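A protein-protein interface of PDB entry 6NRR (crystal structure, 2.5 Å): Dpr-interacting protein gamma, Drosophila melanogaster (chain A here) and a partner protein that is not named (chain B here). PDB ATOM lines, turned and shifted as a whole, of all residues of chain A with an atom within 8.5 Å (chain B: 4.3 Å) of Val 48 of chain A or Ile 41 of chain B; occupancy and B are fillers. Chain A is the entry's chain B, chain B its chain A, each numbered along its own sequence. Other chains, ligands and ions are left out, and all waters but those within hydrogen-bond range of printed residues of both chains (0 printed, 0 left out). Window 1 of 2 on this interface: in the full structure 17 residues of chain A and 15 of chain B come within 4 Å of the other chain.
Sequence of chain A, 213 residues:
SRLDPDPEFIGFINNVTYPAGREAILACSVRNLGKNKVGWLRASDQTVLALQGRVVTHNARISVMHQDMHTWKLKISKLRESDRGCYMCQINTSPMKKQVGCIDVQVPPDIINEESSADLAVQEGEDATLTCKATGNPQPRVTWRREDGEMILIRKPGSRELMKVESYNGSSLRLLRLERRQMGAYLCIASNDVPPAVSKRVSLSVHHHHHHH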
ATOM      1  N   GLY A  39      -1.027  -5.447  -6.725  1.00  0.00           N
ATOM      2  CA  GLY A  39      -2.177  -6.154  -6.196  1.00  0.00           C
ATOM      3  C   GLY A  39      -1.783  -7.065  -5.047  1.00  0.00           C
ATOM      4  O   GLY A  39      -0.633  -7.496  -4.944  1.00  0.00           O
ATOM      5  N   TRP A  40      -2.751  -7.358  -4.178  1.00  0.00           N
ATOM      6  CA  TRP A  40      -2.537  -8.231  -3.031  1.00  0.00           C
ATOM      7  C   TRP A  40      -3.381  -9.492  -3.164  1.00  0.00           C
ATOM      8  O   TRP A  40      -4.540  -9.437  -3.592  1.00  0.00           O
ATOM      9  CB  TRP A  40      -2.875  -7.521  -1.719  1.00  0.00           C
ATOM     10  CG  TRP A  40      -1.829  -6.507  -1.250  1.00  0.00           C
ATOM     11  CD1 TRP A  40      -1.862  -5.154  -1.428  1.00  0.00           C
ATOM     12  CD2 TRP A  40      -0.626  -6.783  -0.518  1.00  0.00           C
ATOM     13  NE1 TRP A  40      -0.759  -4.576  -0.858  1.00  0.00           N
ATOM     14  CE2 TRP A  40       0.018  -5.552  -0.296  1.00  0.00           C
ATOM     15  CE3 TRP A  40      -0.034  -7.953  -0.032  1.00  0.00           C
ATOM     16  CZ2 TRP A  40       1.224  -5.452   0.396  1.00  0.00           C
ATOM     17  CZ3 TRP A  40       1.167  -7.856   0.649  1.00  0.00           C
ATOM     18  CH2 TRP A  40       1.783  -6.611   0.860  1.00  0.00           C
ATOM     19  N   LEU A  41      -2.790 -10.627  -2.793  1.00  0.00           N
ATOM     20  CA  LEU A  41      -3.463 -11.919  -2.858  1.00  0.00           C
ATOM     21  C   LEU A  41      -3.178 -12.672  -1.570  1.00  0.00           C
ATOM     22  O   LEU A  41      -2.012 -12.858  -1.212  1.00  0.00           O
ATOM     23  CB  LEU A  41      -2.985 -12.724  -4.065  1.00  0.00           C
ATOM     24  CG  LEU A  41      -3.602 -14.105  -4.316  1.00  0.00           C
ATOM     25  CD1 LEU A  41      -4.788 -14.028  -5.284  1.00  0.00           C
ATOM     26  CD2 LEU A  41      -2.545 -15.065  -4.830  1.00  0.00           C
ATOM     27  N   ARG A  42      -4.229 -13.083  -0.861  1.00  0.00           N
ATOM     28  CA  ARG A  42      -4.051 -13.963   0.293  1.00  0.00           C
ATOM     29  C   ARG A  42      -3.776 -15.372  -0.209  1.00  0.00           C
ATOM     30  O   ARG A  42      -4.596 -15.945  -0.931  1.00  0.00           O
ATOM     31  CB  ARG A  42      -5.285 -13.948   1.194  1.00  0.00           C
ATOM     32  CG  ARG A  42      -5.127 -14.743   2.485  1.00  0.00           C
ATOM     33  CD  ARG A  42      -6.275 -14.440   3.402  1.00  0.00           C
ATOM     34  NE  ARG A  42      -7.548 -14.724   2.748  1.00  0.00           N
ATOM     35  CZ  ARG A  42      -8.687 -14.096   3.011  1.00  0.00           C
ATOM     36  NH1 ARG A  42      -8.721 -13.128   3.913  1.00  0.00           N
ATOM     37  NH2 ARG A  42      -9.786 -14.430   2.356  1.00  0.00           N
ATOM     38  N   ALA A  43      -2.622 -15.926   0.164  1.00  0.00           N
ATOM     39  CA  ALA A  43      -2.142 -17.143  -0.479  1.00  0.00           C
ATOM     40  C   ALA A  43      -2.864 -18.398   0.008  1.00  0.00           C
ATOM     41  O   ALA A  43      -3.000 -19.362  -0.761  1.00  0.00           O
ATOM     42  CB  ALA A  43      -0.639 -17.286  -0.254  1.00  0.00           C
ATOM     43  N   ASP A  45      -5.999 -19.099   0.637  1.00  0.00           N
ATOM     44  CA  ASP A  45      -7.207 -19.409  -0.117  1.00  0.00           C
ATOM     45  C   ASP A  45      -7.287 -18.624  -1.420  1.00  0.00           C
ATOM     46  O   ASP A  45      -8.388 -18.428  -1.950  1.00  0.00           O
ATOM     47  CB  ASP A  45      -8.456 -19.183   0.745  1.00  0.00           C
ATOM     48  CG  ASP A  45      -8.547 -17.775   1.307  1.00  0.00           C
ATOM     49  OD1 ASP A  45      -7.865 -16.863   0.796  1.00  0.00           O
ATOM     50  OD2 ASP A  45      -9.312 -17.583   2.275  1.00  0.00           O
ATOM     51  N   GLN A  46      -6.137 -18.180  -1.929  1.00  0.00           N
ATOM     52  CA  GLN A  46      -5.983 -17.484  -3.211  1.00  0.00           C
ATOM     53  C   GLN A  46      -7.123 -16.502  -3.454  1.00  0.00           C
ATOM     54  O   GLN A  46      -7.850 -16.560  -4.447  1.00  0.00           O
ATOM     55  CB  GLN A  46      -5.849 -18.481  -4.354  1.00  0.00           C
ATOM     56  CG  GLN A  46      -4.829 -19.544  -4.048  1.00  0.00           C
ATOM     57  CD  GLN A  46      -3.914 -19.812  -5.200  1.00  0.00           C
ATOM     58  OE1 GLN A  46      -4.324 -20.384  -6.210  1.00  0.00           O
ATOM     59  NE2 GLN A  46      -2.660 -19.391  -5.068  1.00  0.00           N
ATOM     60  N   THR A  47      -7.256 -15.589  -2.504  1.00  0.00           N
ATOM     61  CA  THR A  47      -8.307 -14.585  -2.506  1.00  0.00           C
ATOM     62  C   THR A  47      -7.702 -13.236  -2.859  1.00  0.00           C
ATOM     63  O   THR A  47      -6.727 -12.804  -2.235  1.00  0.00           O
ATOM     64  CB  THR A  47      -9.000 -14.502  -1.141  1.00  0.00           C
ATOM     65  OG1 THR A  47      -9.486 -15.802  -0.772  1.00  0.00           O
ATOM     66  CG2 THR A  47     -10.149 -13.502  -1.181  1.00  0.00           C
ATOM     67  N   VAL A  48      -8.284 -12.577  -3.858  1.00  0.00           N
ATOM     68  CA  VAL A  48      -7.882 -11.218  -4.174  1.00  0.00           C
ATOM     69  C   VAL A  48      -8.318 -10.300  -3.045  1.00  0.00           C
ATOM     70  O   VAL A  48      -9.503 -10.250  -2.690  1.00  0.00           O
ATOM     71  CB  VAL A  48      -8.478 -10.780  -5.517  1.00  0.00           C
ATOM     72  CG1 VAL A  48      -8.110  -9.339  -5.814  1.00  0.00           C
ATOM     73  CG2 VAL A  48      -8.002 -11.710  -6.633  1.00  0.00           C
ATOM     74  N   LEU A  49      -7.362  -9.577  -2.466  1.00  0.00           N
ATOM     75  CA  LEU A  49      -7.622  -8.646  -1.371  1.00  0.00           C
ATOM     76  C   LEU A  49      -7.738  -7.201  -1.844  1.00  0.00           C
ATOM     77  O   LEU A  49      -8.700  -6.507  -1.493  1.00  0.00           O
ATOM     78  CB  LEU A  49      -6.518  -8.754  -0.313  1.00  0.00           C
ATOM     79  CG  LEU A  49      -6.290 -10.122   0.324  1.00  0.00           C
ATOM     80  CD1 LEU A  49      -5.460  -9.952   1.570  1.00  0.00           C
ATOM     81  CD2 LEU A  49      -7.619 -10.821   0.653  1.00  0.00           C
ATOM     82  N   ALA A  50      -6.778  -6.725  -2.636  1.00  0.00           N
ATOM     83  CA  ALA A  50      -6.801  -5.334  -3.065  1.00  0.00           C
ATOM     84  C   ALA A  50      -6.109  -5.173  -4.405  1.00  0.00           C
ATOM     85  O   ALA A  50      -5.325  -6.019  -4.842  1.00  0.00           O
ATOM     86  CB  ALA A  50      -6.132  -4.414  -2.049  1.00  0.00           C
ATOM     87  N   LEU A  51      -6.406  -4.046  -5.039  1.00  0.00           N
ATOM     88  CA  LEU A  51      -5.760  -3.634  -6.274  1.00  0.00           C
ATOM     89  C   LEU A  51      -5.487  -2.143  -6.166  1.00  0.00           C
ATOM     90  O   LEU A  51      -6.426  -1.349  -6.023  1.00  0.00           O
ATOM     91  CB  LEU A  51      -6.640  -3.949  -7.488  1.00  0.00           C
ATOM     92  CG  LEU A  51      -6.038  -3.556  -8.827  1.00  0.00           C
ATOM     93  CD1 LEU A  51      -4.606  -4.050  -8.888  1.00  0.00           C
ATOM     94  CD2 LEU A  51      -6.856  -4.137  -9.955  1.00  0.00           C
ATOM     95  N   ARG A  54      -7.360   0.424  -3.720  1.00  0.00           N
ATOM     96  CA  ARG A  54      -8.735   0.019  -3.471  1.00  0.00           C
ATOM     97  C   ARG A  54      -8.792  -1.409  -2.941  1.00  0.00           C
ATOM     98  O   ARG A  54      -8.104  -2.302  -3.446  1.00  0.00           O
ATOM     99  CB  ARG A  54      -9.592   0.153  -4.732  1.00  0.00           C
ATOM    100  CG  ARG A  54     -10.126   1.573  -4.951  1.00  0.00           C
ATOM    101  CD  ARG A  54     -10.645   2.184  -3.638  1.00  0.00           C
ATOM    102  NE  ARG A  54     -11.710   1.385  -3.024  1.00  0.00           N
ATOM    103  CZ  ARG A  54     -11.851   1.192  -1.713  1.00  0.00           C
ATOM    104  NH1 ARG A  54     -10.990   1.727  -0.855  1.00  0.00           N
ATOM    105  NH2 ARG A  54     -12.849   0.451  -1.255  1.00  0.00           N
ATOM    106  N   VAL A  55      -9.615  -1.613  -1.917  1.00  0.00           N
ATOM    107  CA  VAL A  55      -9.807  -2.929  -1.313  1.00  0.00           C
ATOM    108  C   VAL A  55     -10.872  -3.686  -2.095  1.00  0.00           C
ATOM    109  O   VAL A  55     -11.945  -3.150  -2.389  1.00  0.00           O
ATOM    110  CB  VAL A  55     -10.205  -2.801   0.165  1.00  0.00           C
ATOM    111  CG1 VAL A  55     -10.283  -4.172   0.810  1.00  0.00           C
ATOM    112  CG2 VAL A  55      -9.218  -1.908   0.889  1.00  0.00           C
ATOM    113  N   VAL A  56     -10.584  -4.939  -2.426  1.00  0.00           N
ATOM    114  CA  VAL A  56     -11.531  -5.753  -3.184  1.00  0.00           C
ATOM    115  C   VAL A  56     -12.435  -6.557  -2.257  1.00  0.00           C
ATOM    116  O   VAL A  56     -13.660  -6.550  -2.407  1.00  0.00           O
ATOM    117  CB  VAL A  56     -10.769  -6.666  -4.169  1.00  0.00           C
ATOM    118  CG1 VAL A  56     -11.719  -7.625  -4.857  1.00  0.00           C
ATOM    119  CG2 VAL A  56     -10.033  -5.822  -5.196  1.00  0.00           C
ATOM    120  N   THR A  57     -11.841  -7.252  -1.286  1.00  0.00           N
ATOM    121  CA  THR A  57     -12.620  -8.070  -0.369  1.00  0.00           C
ATOM    122  C   THR A  57     -13.563  -7.202   0.450  1.00  0.00           C
ATOM    123  O   THR A  57     -13.233  -6.079   0.839  1.00  0.00           O
ATOM    124  CB  THR A  57     -11.698  -8.873   0.556  1.00  0.00           C
ATOM    125  OG1 THR A  57     -12.491  -9.664   1.454  1.00  0.00           O
ATOM    126  CG2 THR A  57     -10.783  -7.958   1.361  1.00  0.00           C
ATOM    127  N   HIS A  58     -14.759  -7.720   0.690  1.00  0.00           N
ATOM    128  CA  HIS A  58     -15.690  -7.018   1.556  1.00  0.00           C
ATOM    129  C   HIS A  58     -15.433  -7.303   3.025  1.00  0.00           C
ATOM    130  O   HIS A  58     -16.151  -6.780   3.878  1.00  0.00           O
ATOM    131  CB  HIS A  58     -17.131  -7.360   1.167  1.00  0.00           C
ATOM    132  CG  HIS A  58     -17.657  -6.510   0.050  1.00  0.00           C
ATOM    133  ND1 HIS A  58     -17.069  -6.468  -1.197  1.00  0.00           N
ATOM    134  CD2 HIS A  58     -18.697  -5.643   0.003  1.00  0.00           C
ATOM    135  CE1 HIS A  58     -17.736  -5.629  -1.968  1.00  0.00           C
ATOM    136  NE2 HIS A  58     -18.730  -5.115  -1.265  1.00  0.00           N
ATOM    137  N   ASN A  59     -14.416  -8.101   3.333  1.00  0.00           N
ATOM    138  CA  ASN A  59     -13.898  -8.185   4.687  1.00  0.00           C
ATOM    139  C   ASN A  59     -13.596  -6.780   5.199  1.00  0.00           C
ATOM    140  O   ASN A  59     -12.668  -6.112   4.723  1.00  0.00           O
ATOM    141  CB  ASN A  59     -12.653  -9.072   4.715  1.00  0.00           C
ATOM    142  CG  ASN A  59     -12.268  -9.492   6.111  1.00  0.00           C
ATOM    143  OD1 ASN A  59     -12.508  -8.770   7.080  1.00  0.00           O
ATOM    144  ND2 ASN A  59     -11.658 -10.665   6.226  1.00  0.00           N
ATOM    145  N   ILE A  62     -10.020  -5.631   6.632  1.00  0.00           N
ATOM    146  CA  ILE A  62      -8.861  -5.523   5.753  1.00  0.00           C
ATOM    147  C   ILE A  62      -8.936  -4.219   4.966  1.00  0.00           C
ATOM    148  O   ILE A  62     -10.010  -3.826   4.495  1.00  0.00           O
ATOM    149  CB  ILE A  62      -8.767  -6.728   4.802  1.00  0.00           C
ATOM    150  CG1 ILE A  62      -8.918  -8.039   5.587  1.00  0.00           C
ATOM    151  CG2 ILE A  62      -7.442  -6.684   4.042  1.00  0.00           C
ATOM    152  CD1 ILE A  62      -8.723  -9.288   4.753  1.00  0.00           C
ATOM    153  N   LEU A  74      -0.761  -3.302   3.393  1.00  0.00           N
ATOM    154  CA  LEU A  74      -1.945  -4.108   3.664  1.00  0.00           C
ATOM    155  C   LEU A  74      -2.145  -4.178   5.172  1.00  0.00           C
ATOM    156  O   LEU A  74      -1.225  -4.559   5.907  1.00  0.00           O
ATOM    157  CB  LEU A  74      -1.815  -5.522   3.082  1.00  0.00           C
ATOM    158  CG  LEU A  74      -3.058  -6.416   3.066  1.00  0.00           C
ATOM    159  CD1 LEU A  74      -4.109  -5.855   2.136  1.00  0.00           C
ATOM    160  CD2 LEU A  74      -2.693  -7.833   2.646  1.00  0.00           C
ATOM    161  N   MET A  88       0.602 -12.264  -0.806  1.00  0.00           N
ATOM    162  CA  MET A  88       1.403 -12.007  -1.992  1.00  0.00           C
ATOM    163  C   MET A  88       1.143 -10.600  -2.515  1.00  0.00           C
ATOM    164  O   MET A  88       0.000 -10.240  -2.817  1.00  0.00           O
ATOM    165  CB  MET A  88       1.112 -13.035  -3.082  1.00  0.00           C
ATOM    166  CG  MET A  88       1.901 -12.805  -4.352  1.00  0.00           C
ATOM    167  SD  MET A  88       1.653 -14.130  -5.532  1.00  0.00           S
ATOM    168  CE  MET A  88       2.290 -15.515  -4.599  1.00  0.00           C
ATOM    169  N   GLN A  90       1.786  -8.498  -5.683  1.00  0.00           N
ATOM    170  CA  GLN A  90       2.063  -8.746  -7.097  1.00  0.00           C
ATOM    171  C   GLN A  90       2.236  -7.428  -7.843  1.00  0.00           C
ATOM    172  O   GLN A  90       1.413  -6.517  -7.700  1.00  0.00           O
ATOM    173  CB  GLN A  90       0.934  -9.547  -7.755  1.00  0.00           C
ATOM    174  CG  GLN A  90       0.605 -10.863  -7.090  1.00  0.00           C
ATOM    175  CD  GLN A  90      -0.429 -11.666  -7.861  1.00  0.00           C
ATOM    176  OE1 GLN A  90      -1.158 -11.133  -8.702  1.00  0.00           O
ATOM    177  NE2 GLN A  90      -0.489 -12.960  -7.582  1.00  0.00           N
ATOM    178  N   SER B  39     -13.539 -11.193  -9.927  1.00  0.00           N
ATOM    179  CA  SER B  39     -12.125 -11.205 -10.266  1.00  0.00           C
ATOM    180  C   SER B  39     -11.731 -12.553 -10.849  1.00  0.00           C
ATOM    181  O   SER B  39     -12.248 -13.598 -10.434  1.00  0.00           O
ATOM    182  CB  SER B  39     -11.261 -10.907  -9.038  1.00  0.00           C
ATOM    183  OG  SER B  39     -11.715  -9.748  -8.375  1.00  0.00           O
ATOM    184  N   TRP B  40     -10.813 -12.526 -11.811  1.00  0.00           N
ATOM    185  CA  TRP B  40     -10.254 -13.737 -12.389  1.00  0.00           C
ATOM    186  C   TRP B  40      -8.796 -13.861 -11.989  1.00  0.00           C
ATOM    187  O   TRP B  40      -8.054 -12.873 -12.002  1.00  0.00           O
ATOM    188  CB  TRP B  40     -10.376 -13.740 -13.914  1.00  0.00           C
ATOM    189  CG  TRP B  40     -11.752 -14.085 -14.407  1.00  0.00           C
ATOM    190  CD1 TRP B  40     -12.758 -13.212 -14.692  1.00  0.00           C
ATOM    191  CD2 TRP B  40     -12.271 -15.399 -14.666  1.00  0.00           C
ATOM    192  NE1 TRP B  40     -13.865 -13.893 -15.117  1.00  0.00           N
ATOM    193  CE2 TRP B  40     -13.599 -15.240 -15.107  1.00  0.00           C
ATOM    194  CE3 TRP B  40     -11.742 -16.690 -14.567  1.00  0.00           C
ATOM    195  CZ2 TRP B  40     -14.413 -16.326 -15.455  1.00  0.00           C
ATOM    196  CZ3 TRP B  40     -12.551 -17.767 -14.914  1.00  0.00           C
ATOM    197  CH2 TRP B  40     -13.874 -17.574 -15.352  1.00  0.00           C
ATOM    198  N   ILE B  41      -8.394 -15.073 -11.620  1.00  0.00           N
ATOM    199  CA  ILE B  41      -7.011 -15.382 -11.294  1.00  0.00           C
ATOM    200  C   ILE B  41      -6.592 -16.611 -12.081  1.00  0.00           C
ATOM    201  O   ILE B  41      -7.413 -17.468 -12.422  1.00  0.00           O
ATOM    202  CB  ILE B  41      -6.794 -15.614  -9.781  1.00  0.00           C
ATOM    203  CG1 ILE B  41      -7.560 -16.853  -9.300  1.00  0.00           C
ATOM    204  CG2 ILE B  41      -7.212 -14.388  -8.985  1.00  0.00           C
ATOM    205  CD1 ILE B  41      -7.384 -17.131  -7.821  1.00  0.00           C
ATOM    206  N   ARG B  42      -5.299 -16.678 -12.393  1.00  0.00           N
ATOM    207  CA  ARG B  42      -4.701 -17.848 -13.016  1.00  0.00           C
ATOM    208  C   ARG B  42      -4.171 -18.738 -11.903  1.00  0.00           C
ATOM    209  O   ARG B  42      -3.422 -18.272 -11.041  1.00  0.00           O
ATOM    210  CB  ARG B  42      -3.580 -17.438 -13.976  1.00  0.00           C
ATOM    211  CG  ARG B  42      -3.011 -18.566 -14.825  1.00  0.00           C
ATOM    212  CD  ARG B  42      -1.619 -18.223 -15.320  1.00  0.00           C
ATOM    213  NE  ARG B  42      -1.608 -17.221 -16.379  1.00  0.00           N
ATOM    214  CZ  ARG B  42      -0.657 -16.302 -16.525  1.00  0.00           C
ATOM    215  NH1 ARG B  42       0.347 -16.231 -15.664  1.00  0.00           N
ATOM    216  NH2 ARG B  42      -0.725 -15.433 -17.522  1.00  0.00           N
ATOM    217  N   LEU B  43      -4.587 -20.005 -11.901  1.00  0.00           N
ATOM    218  CA  LEU B  43      -4.319 -20.854 -10.742  1.00  0.00           C
ATOM    219  C   LEU B  43      -2.880 -21.349 -10.692  1.00  0.00           C
ATOM    220  O   LEU B  43      -2.354 -21.573  -9.597  1.00  0.00           O
ATOM    221  CB  LEU B  43      -5.285 -22.041 -10.715  1.00  0.00           C
ATOM    222  CG  LEU B  43      -6.648 -21.645 -10.134  1.00  0.00           C
ATOM    223  CD1 LEU B  43      -7.656 -22.789 -10.164  1.00  0.00           C
ATOM    224  CD2 LEU B  43      -6.478 -21.102  -8.720  1.00  0.00           C
ATOM    225  N   HIS B  47      -1.482 -15.593 -10.491  1.00  0.00           N
ATOM    226  CA  HIS B  47      -1.443 -14.279 -11.115  1.00  0.00           C
ATOM    227  C   HIS B  47      -2.840 -13.668 -11.168  1.00  0.00           C
ATOM    228  O   HIS B  47      -3.757 -14.245 -11.757  1.00  0.00           O
ATOM    229  CB  HIS B  47      -0.843 -14.403 -12.519  1.00  0.00           C
ATOM    230  CG  HIS B  47      -0.397 -13.101 -13.115  1.00  0.00           C
ATOM    231  ND1 HIS B  47      -1.128 -11.936 -12.999  1.00  0.00           N
ATOM    232  CD2 HIS B  47       0.700 -12.784 -13.841  1.00  0.00           C
ATOM    233  CE1 HIS B  47      -0.495 -10.958 -13.619  1.00  0.00           C
ATOM    234  NE2 HIS B  47       0.615 -11.447 -14.141  1.00  0.00           N
ATOM    235  N   ILE B  48      -3.005 -12.503 -10.541  1.00  0.00           N
ATOM    236  CA  ILE B  48      -4.254 -11.760 -10.673  1.00  0.00           C
ATOM    237  C   ILE B  48      -4.416 -11.316 -12.121  1.00  0.00           C
ATOM    238  O   ILE B  48      -3.499 -10.743 -12.726  1.00  0.00           O
ATOM    239  CB  ILE B  48      -4.276 -10.558  -9.716  1.00  0.00           C
ATOM    240  CG1 ILE B  48      -4.409 -11.017  -8.261  1.00  0.00           C
ATOM    241  CG2 ILE B  48      -5.402  -9.602 -10.072  1.00  0.00           C
ATOM    242  CD1 ILE B  48      -4.097  -9.931  -7.236  1.00  0.00           C
ATOM    243  N   LEU B  49      -5.582 -11.592 -12.696  1.00  0.00           N
ATOM    244  CA  LEU B  49      -5.837 -11.255 -14.092  1.00  0.00           C
ATOM    245  C   LEU B  49      -6.726 -10.024 -14.228  1.00  0.00           C
ATOM    246  O   LEU B  49      -6.321  -9.019 -14.819  1.00  0.00           O
ATOM    247  CB  LEU B  49      -6.469 -12.447 -14.817  1.00  0.00           C
ATOM    248  CG  LEU B  49      -5.721 -13.771 -14.722  1.00  0.00           C
ATOM    249  CD1 LEU B  49      -6.588 -14.938 -15.204  1.00  0.00           C
ATOM    250  CD2 LEU B  49      -4.410 -13.705 -15.507  1.00  0.00           C
ATOM    251  N   TYR B  87      -8.410 -21.662 -14.503  1.00  0.00           N
ATOM    252  CA  TYR B  87      -8.707 -20.294 -14.131  1.00  0.00           C
ATOM    253  C   TYR B  87      -9.822 -20.316 -13.093  1.00  0.00           C
ATOM    254  O   TYR B  87     -10.651 -21.233 -13.076  1.00  0.00           O
ATOM    255  CB  TYR B  87      -9.094 -19.478 -15.371  1.00  0.00           C
ATOM    256  CG  TYR B  87      -7.959 -19.359 -16.371  1.00  0.00           C
ATOM    257  CD1 TYR B  87      -7.552 -20.449 -17.139  1.00  0.00           C
ATOM    258  CD2 TYR B  87      -7.289 -18.155 -16.541  1.00  0.00           C
ATOM    259  CE1 TYR B  87      -6.506 -20.336 -18.044  1.00  0.00           C
ATOM    260  CE2 TYR B  87      -6.246 -18.031 -17.444  1.00  0.00           C
ATOM    261  CZ  TYR B  87      -5.858 -19.122 -18.190  1.00  0.00           C
ATOM    262  OH  TYR B  87      -4.818 -18.989 -19.082  1.00  0.00           O
ATOM    263  N   GLU B  88      -9.825 -19.326 -12.200  1.00  0.00           N
ATOM    264  CA  GLU B  88     -10.823 -19.261 -11.144  1.00  0.00           C
ATOM    265  C   GLU B  88     -11.492 -17.899 -11.160  1.00  0.00           C
ATOM    266  O   GLU B  88     -10.812 -16.867 -11.155  1.00  0.00           O
ATOM    267  CB  GLU B  88     -10.210 -19.527  -9.763  1.00  0.00           C
ATOM    268  CG  GLU B  88     -11.192 -19.353  -8.592  1.00  0.00           C
ATOM    269  CD  GLU B  88     -10.515 -19.497  -7.245  1.00  0.00           C
ATOM    270  OE1 GLU B  88      -9.741 -20.460  -7.077  1.00  0.00           O
ATOM    271  OE2 GLU B  88     -10.738 -18.642  -6.361  1.00  0.00           O
ATOM    272  N   GLN B  90     -13.912 -15.438  -8.935  1.00  0.00           N
ATOM    273  CA  GLN B  90     -14.232 -15.298  -7.522  1.00  0.00           C
ATOM    274  C   GLN B  90     -14.952 -13.987  -7.253  1.00  0.00           C
ATOM    275  O   GLN B  90     -14.580 -12.936  -7.787  1.00  0.00           O
ATOM    276  CB  GLN B  90     -12.977 -15.398  -6.649  1.00  0.00           C
ATOM    277  CG  GLN B  90     -11.931 -14.338  -6.884  1.00  0.00           C
ATOM    278  CD  GLN B  90     -10.712 -14.563  -6.017  1.00  0.00           C
ATOM    279  OE1 GLN B  90     -10.377 -13.739  -5.163  1.00  0.00           O
ATOM    280  NE2 GLN B  90     -10.045 -15.692  -6.224  1.00  0.00           N
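O of Gln 46 of chain A sits at hydrogen-bond distance from NE2 of Gln 90 of chain B, at 3.0 Å.
The backbone NH of Ile 48 of chain B sits at hydrogen-bond distance from the side-chain amide oxygen of Gln 90 of chain A (2.9 Å).
OE1 of Gln 90 of chain B is in hydrogen-bond range of N of Val 48 of chain A (2.7 Å).
Among the printed residues, pairs that only touch across the chains: Gln 46 of chain A with Leu 43 of chain B (3.4 Å), Gln 46 of chain A with Ile 41 of chain B (3.5 Å), Thr 47 of chain A with Gln 90 of chain B (3.5 Å), Val 48 of chain A with Ile 41 of chain B (3.7 Å), Trp 40 of chain A with Ile 48 of chain B (3.7 Å) and Gln 90 of chain A with His 47 of chain B (3.9 Å).
Of the 11 printed residues of chain B, 5 touch a printed residue of chain A.
Printed residues of chain B that touch a printed residue of chain A: Ile 41, Leu 43, His 47, Ile 48 and Gln 90.
Hydrophobic or aromatic side chains of chain B within 4 Å of the printed part of chain A: Ile 41, Leu 43 and Ile 48.
Along chain B the printed residues that touch a printed residue of chain A span positions 41 to 90.
Printed residues of chain A that touch a printed residue of chain B: Trp 40, Gln 46, Thr 47, Val 48 and Gln 90.
Hydrophobic or aromatic side chains of chain A within 4 Å of the printed part of chain B: Val 48.
Among the printed residues, 9 pairs touch across the chains.
Of the printed residues of chain B, Trp 40 of chain A touches Ile 48.
Printed residues of chain B within 4 Å of Thr 47 of chain A: Gln 90.
Of the printed residues of chain B, Gln 90 of chain A touches His 47 and Ile 48.
Of the printed residues of chain A, Ile 41 of chain B touches Gln 46 and Val 48.
Printed residues of chain A within 4 Å of Leu 43 of chain B: Gln 46 (3.4 Å).
Printed residues of chain A within 4 Å of His 47 of chain B: Gln 90.
The nearest printed residue of chain B that does not touch Val 48 of chain A is Ile 48 of chain B (4.01 Å).
The nearest printed residue of chain A that does not touch Ile 48 of chain B is Val 48 of chain A (4.01 Å).
The backbone carbonyl oxygen of Thr 47 of chain A sits at hydrogen-bond distance from the backbone NH of Arg 42 of chain A (2.9 Å).
The backbone NH (N) of Trp 40 of chain A sits at hydrogen-bond distance from the backbone carbonyl oxygen (O) of Ala 50 of chain A.
The backbone NH (N) of Ile 41 of chain B lies within hydrogen-bond range of the backbone carbonyl oxygen (O) of Glu 88 of chain B, at 3.0 Å.
The side-chain amide nitrogen (NE2) of Gln 90 of chain A lies within hydrogen-bond range of the side-chain sulfur (SD) of Met 88 of chain A, at 3.2 Å.
The backbone carbonyl oxygen (O) of Trp 40 of chain A sits at hydrogen-bond distance from the backbone NH (N) of Leu 49 of chain A (3.0 Å).
The backbone NH (N) of Arg 42 of chain B is in hydrogen-bond range of the backbone carbonyl oxygen (O) of His 47 of chain B (2.9 Å).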
